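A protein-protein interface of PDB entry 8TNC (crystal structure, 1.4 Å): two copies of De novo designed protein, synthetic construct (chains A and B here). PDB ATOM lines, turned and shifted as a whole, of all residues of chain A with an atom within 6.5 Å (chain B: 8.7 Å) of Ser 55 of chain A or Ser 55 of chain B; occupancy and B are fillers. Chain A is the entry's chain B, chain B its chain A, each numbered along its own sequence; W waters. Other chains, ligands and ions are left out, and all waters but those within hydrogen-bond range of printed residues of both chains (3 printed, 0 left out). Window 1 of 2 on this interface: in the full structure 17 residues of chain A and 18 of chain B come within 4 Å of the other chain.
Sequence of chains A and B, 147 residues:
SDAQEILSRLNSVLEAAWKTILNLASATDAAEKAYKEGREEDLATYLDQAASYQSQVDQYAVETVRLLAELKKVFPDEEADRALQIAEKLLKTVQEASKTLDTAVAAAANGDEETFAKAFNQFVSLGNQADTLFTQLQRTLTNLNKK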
ATOM      1  N   ALA A  50      28.932 -17.529   4.914  1.00  0.00           N
ATOM      2  CA  ALA A  50      27.994 -18.328   5.691  1.00  0.00           C
ATOM      3  C   ALA A  50      27.548 -17.588   6.944  1.00  0.00           C
ATOM      4  O   ALA A  50      26.356 -17.584   7.276  1.00  0.00           O
ATOM      5  CB  ALA A  50      28.655 -19.646   6.077  1.00  0.00           C
ATOM      6  N   ALA A  51      28.481 -16.959   7.647  1.00  0.00           N
ATOM      7  CA  ALA A  51      28.122 -16.242   8.863  1.00  0.00           C
ATOM      8  C   ALA A  51      27.152 -15.115   8.561  1.00  0.00           C
ATOM      9  O   ALA A  51      26.210 -14.876   9.334  1.00  0.00           O
ATOM     10  CB  ALA A  51      29.388 -15.708   9.499  1.00  0.00           C
ATOM     11  N   SER A  52      27.345 -14.414   7.445  1.00  0.00           N
ATOM     12  CA  SER A  52      26.436 -13.326   7.099  1.00  0.00           C
ATOM     13  C   SER A  52      25.046 -13.854   6.798  1.00  0.00           C
ATOM     14  O   SER A  52      24.034 -13.310   7.277  1.00  0.00           O
ATOM     15  CB  SER A  52      27.003 -12.558   5.918  1.00  0.00           C
ATOM     16  OG  SER A  52      26.113 -11.525   5.503  1.00  0.00           O
ATOM     17  N   TYR A  53      24.952 -14.939   6.029  1.00  0.00           N
ATOM     18  CA  TYR A  53      23.639 -15.512   5.754  1.00  0.00           C
ATOM     19  C   TYR A  53      22.985 -16.056   7.020  1.00  0.00           C
ATOM     20  O   TYR A  53      21.772 -15.897   7.212  1.00  0.00           O
ATOM     21  CB  TYR A  53      23.737 -16.608   4.699  1.00  0.00           C
ATOM     22  CG  TYR A  53      24.168 -16.136   3.317  1.00  0.00           C
ATOM     23  CD1 TYR A  53      23.526 -15.071   2.676  1.00  0.00           C
ATOM     24  CD2 TYR A  53      25.192 -16.792   2.642  1.00  0.00           C
ATOM     25  CE1 TYR A  53      23.938 -14.643   1.397  1.00  0.00           C
ATOM     26  CE2 TYR A  53      25.582 -16.395   1.386  1.00  0.00           C
ATOM     27  CZ  TYR A  53      24.968 -15.329   0.775  1.00  0.00           C
ATOM     28  OH  TYR A  53      25.383 -14.943  -0.492  1.00  0.00           O
ATOM     29  N   GLN A  54      23.759 -16.687   7.893  1.00  0.00           N
ATOM     30  CA  GLN A  54      23.210 -17.178   9.149  1.00  0.00           C
ATOM     31  C   GLN A  54      22.639 -16.033   9.973  1.00  0.00           C
ATOM     32  O   GLN A  54      21.576 -16.174  10.585  1.00  0.00           O
ATOM     33  CB  GLN A  54      24.291 -17.962   9.907  1.00  0.00           C
ATOM     34  CG  GLN A  54      23.824 -18.526  11.259  1.00  0.00           C
ATOM     35  CD  GLN A  54      22.790 -19.604  11.090  1.00  0.00           C
ATOM     36  OE1 GLN A  54      23.119 -20.726  10.751  1.00  0.00           O
ATOM     37  NE2 GLN A  54      21.537 -19.277  11.310  1.00  0.00           N
ATOM     38  N   SER A  55      23.339 -14.898  10.032  1.00  0.00           N
ATOM     39  CA  SER A  55      22.794 -13.766  10.786  1.00  0.00           C
ATOM     40  C   SER A  55      21.481 -13.290  10.200  1.00  0.00           C
ATOM     41  O   SER A  55      20.562 -12.896  10.944  1.00  0.00           O
ATOM     42  CB  SER A  55      23.799 -12.618  10.799  1.00  0.00           C
ATOM     43  OG  SER A  55      24.850 -12.961  11.678  1.00  0.00           O
ATOM     44  N   GLN A  56      21.350 -13.310   8.874  1.00  0.00           N
ATOM     45  CA  GLN A  56      20.104 -12.915   8.243  1.00  0.00           C
ATOM     46  C   GLN A  56      18.989 -13.916   8.543  1.00  0.00           C
ATOM     47  O   GLN A  56      17.849 -13.516   8.806  1.00  0.00           O
ATOM     48  CB  GLN A  56      20.314 -12.764   6.738  1.00  0.00           C
ATOM     49  CG  GLN A  56      21.232 -11.636   6.287  1.00  0.00           C
ATOM     50  CD  GLN A  56      21.717 -11.834   4.839  1.00  0.00           C
ATOM     51  OE1 GLN A  56      20.939 -12.179   3.952  1.00  0.00           O
ATOM     52  NE2 GLN A  56      23.004 -11.590   4.602  1.00  0.00           N
ATOM     53  N   VAL A  57      19.275 -15.220   8.502  1.00  0.00           N
ATOM     54  CA  VAL A  57      18.261 -16.205   8.897  1.00  0.00           C
ATOM     55  C   VAL A  57      17.824 -15.981  10.340  1.00  0.00           C
ATOM     56  O   VAL A  57      16.638 -16.130  10.665  1.00  0.00           O
ATOM     57  CB  VAL A  57      18.804 -17.635   8.712  1.00  0.00           C
ATOM     58  CG1 VAL A  57      17.799 -18.680   9.212  1.00  0.00           C
ATOM     59  CG2 VAL A  57      19.140 -17.906   7.244  1.00  0.00           C
ATOM     60  N   ASP A  58      18.773 -15.660  11.229  1.00  0.00           N
ATOM     61  CA  ASP A  58      18.463 -15.370  12.635  1.00  0.00           C
ATOM     62  C   ASP A  58      17.419 -14.255  12.710  1.00  0.00           C
ATOM     63  O   ASP A  58      16.390 -14.356  13.411  1.00  0.00           O
ATOM     64  CB  ASP A  58      19.750 -14.870  13.330  1.00  0.00           C
ATOM     65  CG  ASP A  58      20.835 -15.940  13.572  1.00  0.00           C
ATOM     66  OD1 ASP A  58      20.599 -17.145  13.352  1.00  0.00           O
ATOM     67  OD2 ASP A  58      21.995 -15.550  13.967  1.00  0.00           O
ATOM     68  N   GLN A  59      17.641 -13.189  11.944  1.00  0.00           N
ATOM     69  CA  GLN A  59      16.724 -12.054  11.954  1.00  0.00           C
ATOM     70  C   GLN A  59      15.347 -12.453  11.438  1.00  0.00           C
ATOM     71  O   GLN A  59      14.321 -12.083  12.027  1.00  0.00           O
ATOM     72  CB  GLN A  59      17.310 -10.918  11.129  1.00  0.00           C
ATOM     73  CG  GLN A  59      16.375  -9.727  10.962  1.00  0.00           C
ATOM     74  CD  GLN A  59      16.032  -9.090  12.280  1.00  0.00           C
ATOM     75  OE1 GLN A  59      16.883  -8.975  13.167  1.00  0.00           O
ATOM     76  NE2 GLN A  59      14.768  -8.679  12.429  1.00  0.00           N
ATOM     77  N   TYR A  60      15.291 -13.204  10.349  1.00  0.00           N
ATOM     78  CA  TYR A  60      13.995 -13.615   9.823  1.00  0.00           C
ATOM     79  C   TYR A  60      13.280 -14.546  10.792  1.00  0.00           C
ATOM     80  O   TYR A  60      12.042 -14.508  10.885  1.00  0.00           O
ATOM     81  CB  TYR A  60      14.153 -14.319   8.477  1.00  0.00           C
ATOM     82  CG  TYR A  60      14.530 -13.439   7.316  1.00  0.00           C
ATOM     83  CD1 TYR A  60      13.923 -12.220   7.084  1.00  0.00           C
ATOM     84  CD2 TYR A  60      15.525 -13.848   6.454  1.00  0.00           C
ATOM     85  CE1 TYR A  60      14.298 -11.429   6.004  1.00  0.00           C
ATOM     86  CE2 TYR A  60      15.900 -13.092   5.382  1.00  0.00           C
ATOM     87  CZ  TYR A  60      15.297 -11.875   5.156  1.00  0.00           C
ATOM     88  OH  TYR A  60      15.706 -11.109   4.076  1.00  0.00           O
ATOM     89  N   SER A  98      23.501 -20.962  14.886  1.00  0.00           N
ATOM     90  CA  SER A  98      24.281 -19.739  14.742  1.00  0.00           C
ATOM     91  C   SER A  98      25.465 -19.722  15.690  1.00  0.00           C
ATOM     92  O   SER A  98      26.589 -19.367  15.290  1.00  0.00           O
ATOM     93  CB  SER A  98      23.370 -18.547  15.019  1.00  0.00           C
ATOM     94  OG  SER A  98      24.070 -17.353  14.746  1.00  0.00           O
ATOM     95  N   ASP A 102      29.420 -19.924  14.717  1.00  0.00           N
ATOM     96  CA  ASP A 102      30.366 -18.935  15.240  1.00  0.00           C
ATOM     97  C   ASP A 102      31.598 -19.606  15.829  1.00  0.00           C
ATOM     98  O   ASP A 102      32.734 -19.153  15.598  1.00  0.00           O
ATOM     99  CB  ASP A 102      29.690 -18.061  16.298  1.00  0.00           C
ATOM    100  CG  ASP A 102      29.447 -16.628  15.819  1.00  0.00           C
ATOM    101  OD1 ASP A 102      29.358 -15.729  16.694  1.00  0.00           O
ATOM    102  OD2 ASP A 102      29.366 -16.393  14.589  1.00  0.00           O
ATOM    103  N   THR B  20      31.485   0.813  15.125  1.00  0.00           N
ATOM    104  CA  THR B  20      30.392  -0.139  15.307  1.00  0.00           C
ATOM    105  C   THR B  20      30.086  -0.348  16.784  1.00  0.00           C
ATOM    106  O   THR B  20      28.918  -0.472  17.150  1.00  0.00           O
ATOM    107  CB  THR B  20      30.773  -1.454  14.613  1.00  0.00           C
ATOM    108  OG1 THR B  20      31.027  -1.184  13.224  1.00  0.00           O
ATOM    109  CG2 THR B  20      29.680  -2.491  14.722  1.00  0.00           C
ATOM    110  N   LEU B  24      26.600   0.068  18.707  1.00  0.00           N
ATOM    111  CA  LEU B  24      26.035  -0.993  19.543  1.00  0.00           C
ATOM    112  C   LEU B  24      25.680  -0.460  20.921  1.00  0.00           C
ATOM    113  O   LEU B  24      24.601  -0.788  21.467  1.00  0.00           O
ATOM    114  CB  LEU B  24      27.032  -2.165  19.638  1.00  0.00           C
ATOM    115  CG  LEU B  24      26.637  -3.309  20.567  1.00  0.00           C
ATOM    116  CD1 LEU B  24      25.311  -3.922  20.131  1.00  0.00           C
ATOM    117  CD2 LEU B  24      27.752  -4.369  20.620  1.00  0.00           C
ATOM    118  N   ASP B  48      16.801  -5.405  17.389  1.00  0.00           N
ATOM    119  CA  ASP B  48      17.242  -5.826  16.061  1.00  0.00           C
ATOM    120  C   ASP B  48      18.437  -5.005  15.602  1.00  0.00           C
ATOM    121  O   ASP B  48      19.373  -5.546  14.994  1.00  0.00           O
ATOM    122  CB  ASP B  48      16.130  -5.698  15.049  1.00  0.00           C
ATOM    123  CG  ASP B  48      15.109  -6.810  15.179  1.00  0.00           C
ATOM    124  OD1 ASP B  48      14.014  -6.671  14.592  1.00  0.00           O
ATOM    125  OD2 ASP B  48      15.375  -7.790  15.927  1.00  0.00           O
ATOM    126  N   GLN B  49      18.441  -3.703  15.867  1.00  0.00           N
ATOM    127  CA  GLN B  49      19.596  -2.873  15.523  1.00  0.00           C
ATOM    128  C   GLN B  49      20.828  -3.323  16.293  1.00  0.00           C
ATOM    129  O   GLN B  49      21.925  -3.473  15.726  1.00  0.00           O
ATOM    130  CB  GLN B  49      19.297  -1.412  15.846  1.00  0.00           C
ATOM    131  CG  GLN B  49      18.314  -0.741  14.942  1.00  0.00           C
ATOM    132  CD  GLN B  49      18.844  -0.521  13.528  1.00  0.00           C
ATOM    133  OE1 GLN B  49      19.954  -0.029  13.334  1.00  0.00           O
ATOM    134  NE2 GLN B  49      18.044  -0.876  12.549  1.00  0.00           N
ATOM    135  N   ALA B  50      20.673  -3.568  17.582  1.00  0.00           N
ATOM    136  CA  ALA B  50      21.777  -4.070  18.395  1.00  0.00           C
ATOM    137  C   ALA B  50      22.321  -5.378  17.846  1.00  0.00           C
ATOM    138  O   ALA B  50      23.544  -5.550  17.748  1.00  0.00           O
ATOM    139  CB  ALA B  50      21.324  -4.226  19.848  1.00  0.00           C
ATOM    140  N   ALA B  51      21.443  -6.320  17.488  1.00  0.00           N
ATOM    141  CA  ALA B  51      21.918  -7.583  16.943  1.00  0.00           C
ATOM    142  C   ALA B  51      22.689  -7.387  15.642  1.00  0.00           C
ATOM    143  O   ALA B  51      23.679  -8.099  15.382  1.00  0.00           O
ATOM    144  CB  ALA B  51      20.750  -8.541  16.762  1.00  0.00           C
ATOM    145  N   SER B  52      22.277  -6.429  14.821  1.00  0.00           N
ATOM    146  CA  SER B  52      22.982  -6.210  13.562  1.00  0.00           C
ATOM    147  C   SER B  52      24.376  -5.645  13.826  1.00  0.00           C
ATOM    148  O   SER B  52      25.377  -6.101  13.241  1.00  0.00           O
ATOM    149  CB  SER B  52      22.172  -5.273  12.675  1.00  0.00           C
ATOM    150  OG  SER B  52      22.933  -4.836  11.565  1.00  0.00           O
ATOM    151  N   TYR B  53      24.495  -4.678  14.741  1.00  0.00           N
ATOM    152  CA  TYR B  53      25.821  -4.161  15.088  1.00  0.00           C
ATOM    153  C   TYR B  53      26.681  -5.225  15.751  1.00  0.00           C
ATOM    154  O   TYR B  53      27.886  -5.316  15.467  1.00  0.00           O
ATOM    155  CB  TYR B  53      25.718  -2.930  15.980  1.00  0.00           C
ATOM    156  CG  TYR B  53      25.087  -1.727  15.333  1.00  0.00           C
ATOM    157  CD1 TYR B  53      25.541  -1.229  14.116  1.00  0.00           C
ATOM    158  CD2 TYR B  53      24.043  -1.065  15.975  1.00  0.00           C
ATOM    159  CE1 TYR B  53      24.938  -0.116  13.538  1.00  0.00           C
ATOM    160  CE2 TYR B  53      23.446   0.050  15.413  1.00  0.00           C
ATOM    161  CZ  TYR B  53      23.895   0.507  14.200  1.00  0.00           C
ATOM    162  OH  TYR B  53      23.305   1.628  13.640  1.00  0.00           O
ATOM    163  N   GLN B  54      26.095  -6.056  16.607  1.00  0.00           N
ATOM    164  CA  GLN B  54      26.857  -7.129  17.236  1.00  0.00           C
ATOM    165  C   GLN B  54      27.400  -8.094  16.188  1.00  0.00           C
ATOM    166  O   GLN B  54      28.541  -8.555  16.298  1.00  0.00           O
ATOM    167  CB  GLN B  54      25.926  -7.849  18.223  1.00  0.00           C
ATOM    168  CG  GLN B  54      26.610  -9.011  18.972  1.00  0.00           C
ATOM    169  CD  GLN B  54      27.726  -8.536  19.875  1.00  0.00           C
ATOM    170  OE1 GLN B  54      27.483  -8.048  20.971  1.00  0.00           O
ATOM    171  NE2 GLN B  54      28.976  -8.658  19.421  1.00  0.00           N
ATOM    172  N   SER B  55      26.590  -8.425  15.187  1.00  0.00           N
ATOM    173  CA  SER B  55      27.057  -9.296  14.105  1.00  0.00           C
ATOM    174  C   SER B  55      28.262  -8.685  13.392  1.00  0.00           C
ATOM    175  O   SER B  55      29.229  -9.396  13.049  1.00  0.00           O
ATOM    176  CB  SER B  55      25.911  -9.577  13.129  1.00  0.00           C
ATOM    177  OG  SER B  55      26.347 -10.579  12.241  1.00  0.00           O
ATOM    178  N   GLN B  56      28.257  -7.366  13.200  1.00  0.00           N
ATOM    179  CA  GLN B  56      29.370  -6.700  12.532  1.00  0.00           C
ATOM    180  C   GLN B  56      30.609  -6.699  13.418  1.00  0.00           C
ATOM    181  O   GLN B  56      31.728  -6.891  12.912  1.00  0.00           O
ATOM    182  CB  GLN B  56      28.943  -5.276  12.146  1.00  0.00           C
ATOM    183  CG  GLN B  56      30.002  -4.481  11.360  1.00  0.00           C
ATOM    184  CD  GLN B  56      30.526  -5.208  10.084  1.00  0.00           C
ATOM    185  OE1 GLN B  56      31.613  -5.835  10.071  1.00  0.00           O
ATOM    186  NE2 GLN B  56      29.756  -5.102   9.003  1.00  0.00           N
ATOM    187  N   VAL B  57      30.457  -6.481  14.728  1.00  0.00           N
ATOM    188  CA  VAL B  57      31.600  -6.590  15.649  1.00  0.00           C
ATOM    189  C   VAL B  57      32.192  -7.990  15.603  1.00  0.00           C
ATOM    190  O   VAL B  57      33.416  -8.157  15.563  1.00  0.00           O
ATOM    191  CB  VAL B  57      31.236  -6.167  17.087  1.00  0.00           C
ATOM    192  CG1 VAL B  57      32.465  -6.300  18.033  1.00  0.00           C
ATOM    193  CG2 VAL B  57      30.707  -4.714  17.114  1.00  0.00           C
ATOM    194  N   ASP B  58      31.347  -9.015  15.588  1.00  0.00           N
ATOM    195  CA  ASP B  58      31.803 -10.390  15.464  1.00  0.00           C
ATOM    196  C   ASP B  58      32.675 -10.541  14.215  1.00  0.00           C
ATOM    197  O   ASP B  58      33.774 -11.089  14.280  1.00  0.00           O
ATOM    198  CB  ASP B  58      30.615 -11.374  15.346  1.00  0.00           C
ATOM    199  CG  ASP B  58      29.581 -11.334  16.482  1.00  0.00           C
ATOM    200  OD1 ASP B  58      29.849 -10.868  17.600  1.00  0.00           O
ATOM    201  OD2 ASP B  58      28.455 -11.851  16.231  1.00  0.00           O
ATOM    202  N   GLN B  59      32.231  -9.996  13.083  1.00  0.00           N
ATOM    203  CA  GLN B  59      33.001 -10.148  11.853  1.00  0.00           C
ATOM    204  C   GLN B  59      34.347  -9.444  11.970  1.00  0.00           C
ATOM    205  O   GLN B  59      35.386  -9.988  11.556  1.00  0.00           O
ATOM    206  CB  GLN B  59      32.204  -9.607  10.678  1.00  0.00           C
ATOM    207  CG  GLN B  59      32.990  -9.522   9.377  1.00  0.00           C
ATOM    208  CD  GLN B  59      33.384 -10.880   8.867  1.00  0.00           C
ATOM    209  OE1 GLN B  59      32.653 -11.862   9.048  1.00  0.00           O
ATOM    210  NE2 GLN B  59      34.573 -10.963   8.258  1.00  0.00           N
ATOM    211  N   TYR B  60      34.375  -8.239  12.538  1.00  0.00           N
ATOM    212  CA  TYR B  60      35.644  -7.536  12.701  1.00  0.00           C
ATOM    213  C   TYR B  60      36.572  -8.263  13.660  1.00  0.00           C
ATOM    214  O   TYR B  60      37.806  -8.232  13.483  1.00  0.00           O
ATOM    215  CB  TYR B  60      35.406  -6.114  13.215  1.00  0.00           C
ATOM    216  CG  TYR B  60      34.810  -5.145  12.230  1.00  0.00           C
ATOM    217  CD1 TYR B  60      35.273  -5.052  10.934  1.00  0.00           C
ATOM    218  CD2 TYR B  60      33.784  -4.302  12.620  1.00  0.00           C
ATOM    219  CE1 TYR B  60      34.726  -4.148  10.034  1.00  0.00           C
ATOM    220  CE2 TYR B  60      33.246  -3.394  11.743  1.00  0.00           C
ATOM    221  CZ  TYR B  60      33.706  -3.319  10.452  1.00  0.00           C
ATOM    222  OH  TYR B  60      33.151  -2.411   9.562  1.00  0.00           O
ATOM    223  N   ALA B  61      36.033  -8.870  14.707  1.00  0.00           N
ATOM    224  CA  ALA B  61      36.853  -9.596  15.666  1.00  0.00           C
ATOM    225  C   ALA B  61      37.489 -10.836  15.040  1.00  0.00           C
ATOM    226  O   ALA B  61      38.644 -11.194  15.346  1.00  0.00           O
ATOM    227  CB  ALA B  61      36.022  -9.983  16.885  1.00  0.00           C
ATOM    228  N   VAL B  62      36.750 -11.505  14.157  1.00  0.00           N
ATOM    229  CA  VAL B  62      37.305 -12.619  13.388  1.00  0.00           C
ATOM    230  C   VAL B  62      38.425 -12.127  12.483  1.00  0.00           C
ATOM    231  O   VAL B  62      39.515 -12.732  12.414  1.00  0.00           O
ATOM    232  CB  VAL B  62      36.187 -13.305  12.582  1.00  0.00           C
ATOM    233  CG1 VAL B  62      36.801 -14.332  11.587  1.00  0.00           C
ATOM    234  CG2 VAL B  62      35.245 -13.998  13.519  1.00  0.00           C
ATOM    235  N   GLU B  63      38.187 -11.032  11.768  1.00  0.00           N
ATOM    236  CA  GLU B  63      39.194 -10.490  10.855  1.00  0.00           C
ATOM    237  C   GLU B  63      40.448 -10.099  11.616  1.00  0.00           C
ATOM    238  O   GLU B  63      41.578 -10.301  11.139  1.00  0.00           O
ATOM    239  CB  GLU B  63      38.644  -9.260  10.141  1.00  0.00           C
ATOM    240  CG  GLU B  63      37.680  -9.555   9.030  1.00  0.00           C
ATOM    241  CD  GLU B  63      36.981  -8.307   8.523  1.00  0.00           C
ATOM    242  OE1 GLU B  63      37.610  -7.224   8.510  1.00  0.00           O
ATOM    243  OE2 GLU B  63      35.823  -8.425   8.067  1.00  0.00           O
ATOM    244  N   VAL B  94      33.463 -11.571  22.583  1.00  0.00           N
ATOM    245  CA  VAL B  94      32.523 -11.054  21.590  1.00  0.00           C
ATOM    246  C   VAL B  94      31.488 -12.104  21.213  1.00  0.00           C
ATOM    247  O   VAL B  94      30.281 -11.820  21.142  1.00  0.00           O
ATOM    248  CB  VAL B  94      33.294 -10.542  20.360  1.00  0.00           C
ATOM    249  CG1 VAL B  94      32.357 -10.286  19.217  1.00  0.00           C
ATOM    250  CG2 VAL B  94      34.055  -9.289  20.713  1.00  0.00           C
ATOM    251  N   GLN B  95      31.931 -13.342  20.967  1.00  0.00           N
ATOM    252  CA  GLN B  95      30.992 -14.390  20.594  1.00  0.00           C
ATOM    253  C   GLN B  95      30.087 -14.787  21.753  1.00  0.00           C
ATOM    254  O   GLN B  95      28.919 -15.128  21.520  1.00  0.00           O
ATOM    255  CB  GLN B  95      31.753 -15.566  19.995  1.00  0.00           C
ATOM    256  CG  GLN B  95      32.395 -15.186  18.657  1.00  0.00           C
ATOM    257  CD  GLN B  95      32.869 -16.414  17.893  1.00  0.00           C
ATOM    258  OE1 GLN B  95      33.161 -17.450  18.485  1.00  0.00           O
ATOM    259  NE2 GLN B  95      32.911 -16.302  16.586  1.00  0.00           N
ATOM    260  N   ALA B  97      29.109 -12.569  24.067  1.00  0.00           N
ATOM    261  CA  ALA B  97      28.161 -11.451  24.046  1.00  0.00           C
ATOM    262  C   ALA B  97      27.120 -11.656  22.955  1.00  0.00           C
ATOM    263  O   ALA B  97      25.926 -11.422  23.164  1.00  0.00           O
ATOM    264  CB  ALA B  97      28.891 -10.131  23.852  1.00  0.00           C
ATOM    265  N   SER B  98      27.540 -12.131  21.784  1.00  0.00           N
ATOM    266  CA  SER B  98      26.608 -12.307  20.673  1.00  0.00           C
ATOM    267  C   SER B  98      25.548 -13.370  20.961  1.00  0.00           C
ATOM    268  O   SER B  98      24.347 -13.157  20.690  1.00  0.00           O
ATOM    269  CB  SER B  98      27.420 -12.645  19.421  1.00  0.00           C
ATOM    270  OG  SER B  98      26.585 -12.694  18.283  1.00  0.00           O
ATOM    271  N   LEU B 101      23.129 -11.923  23.658  1.00  0.00           N
ATOM    272  CA  LEU B 101      22.196 -10.974  23.058  1.00  0.00           C
ATOM    273  C   LEU B 101      21.145 -11.710  22.239  1.00  0.00           C
ATOM    274  O   LEU B 101      19.956 -11.368  22.285  1.00  0.00           O
ATOM    275  CB  LEU B 101      22.954  -9.974  22.191  1.00  0.00           C
ATOM    276  CG  LEU B 101      22.165  -8.863  21.526  1.00  0.00           C
ATOM    277  CD1 LEU B 101      21.389  -8.043  22.576  1.00  0.00           C
ATOM    278  CD2 LEU B 101      22.995  -7.988  20.650  1.00  0.00           C
ATOM    279  N   ASP B 102      21.536 -12.765  21.524  1.00  0.00           N
ATOM    280  CA  ASP B 102      20.561 -13.521  20.744  1.00  0.00           C
ATOM    281  C   ASP B 102      19.507 -14.140  21.651  1.00  0.00           C
ATOM    282  O   ASP B 102      18.313 -14.111  21.337  1.00  0.00           O
ATOM    283  CB  ASP B 102      21.286 -14.604  19.950  1.00  0.00           C
ATOM    284  CG  ASP B 102      21.731 -14.126  18.571  1.00  0.00           C
ATOM    285  OD1 ASP B 102      21.120 -13.181  18.011  1.00  0.00           O
ATOM    286  OD2 ASP B 102      22.703 -14.706  18.046  1.00  0.00           O
ATOM    287  N   PHE B 123      24.649  -9.853  28.908  1.00  0.00           N
ATOM    288  CA  PHE B 123      25.212  -9.216  27.722  1.00  0.00           C
ATOM    289  C   PHE B 123      25.955  -7.948  28.106  1.00  0.00           C
ATOM    290  O   PHE B 123      27.073  -7.718  27.633  1.00  0.00           O
ATOM    291  CB  PHE B 123      24.109  -8.903  26.702  1.00  0.00           C
ATOM    292  CG  PHE B 123      24.528  -7.899  25.673  1.00  0.00           C
ATOM    293  CD1 PHE B 123      25.315  -8.271  24.581  1.00  0.00           C
ATOM    294  CD2 PHE B 123      24.183  -6.569  25.818  1.00  0.00           C
ATOM    295  CE1 PHE B 123      25.695  -7.338  23.644  1.00  0.00           C
ATOM    296  CE2 PHE B 123      24.587  -5.629  24.885  1.00  0.00           C
ATOM    297  CZ  PHE B 123      25.353  -6.025  23.798  1.00  0.00           C
HETATM  298  O   HOH W   1      28.295 -17.000  19.481  1.00  0.00           O
HETATM  299  O   HOH W   2      19.112  -7.858  13.355  1.00  0.00           O
HETATM  300  O   HOH W   3      17.299  -9.794  15.528  1.00  0.00           O
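Ser 55 of chain A touches just one residue of chain B: Ser 55 (2.9 Å). Printed residues of chain B within 4 Å of Gln 59 of chain A: Asp 48 (3.0 Å). Ser 55 of chain B touches just one residue of chain A: Ser 55. Glu 63 of chain B touches none of the printed residues of chain A. Of the printed residues of chain A, Gln 95 of chain B touches Asp 102. Ser 98 of chain B touches none of the printed residues of chain A. The nearest residue of chain B that does not touch Ser 55 of chain A is Asp 58 of chain B (5.9 Å). The nearest residue of chain A that does not touch Ser 55 of chain B is Ala 51 of chain A (5.2 Å). The nearest printed residue of chain A that does not touch Asp 48 of chain B is Asp 58 of chain A (7.1 Å).
Of the 25 printed residues of chain B, 3 touch a printed residue of chain A. Printed residues of chain B that touch a printed residue of chain A: Asp 48, Ser 55 and Gln 95. Of the 13 printed residues of chain A, 3 touch a printed residue of chain B. Among the printed residues, 3 pairs touch across the chains.
The side-chain carboxylate (OD1) of Asp 48 of chain B lies within hydrogen-bond range of the side-chain amide nitrogen (NE2) of Gln 59 of chain A (3.0 Å). The side-chain hydroxyl of Ser 55 of chain B lies within hydrogen-bond range of the side-chain hydroxyl of Ser 55 of chain A, 2.9 Å away. NE2 of Gln 95 of chain B sits at hydrogen-bond distance from O of Asp 102 of chain A (3.0 Å).
O of Ala 51 of chain A lies within hydrogen-bond range of OG of Ser 55 of chain A.
Ser 55 of chain A touches its own counterpart, Ser 55 of chain B. Of the 3 pairs that touch across the chains among the printed residues, 1 has its exchanged pair printed and touching as well.
Water W2 lies within hydrogen-bond range of the side-chain amide oxygen of Gln 59 of chain A (2.5 Å) and the backbone carbonyl oxygen of Asp 48 of chain B (2.8 Å). Water W3 bridges the side-chain amide oxygen of Gln 59 of chain A (2.5 Å) and the side-chain carboxylate of Asp 48 of chain B (2.8 Å). Water W1 lies within hydrogen-bond range of O of Gln 95 of chain B (2.8 Å) and OD1 of Asp 102 of chain A (3.2 Å).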
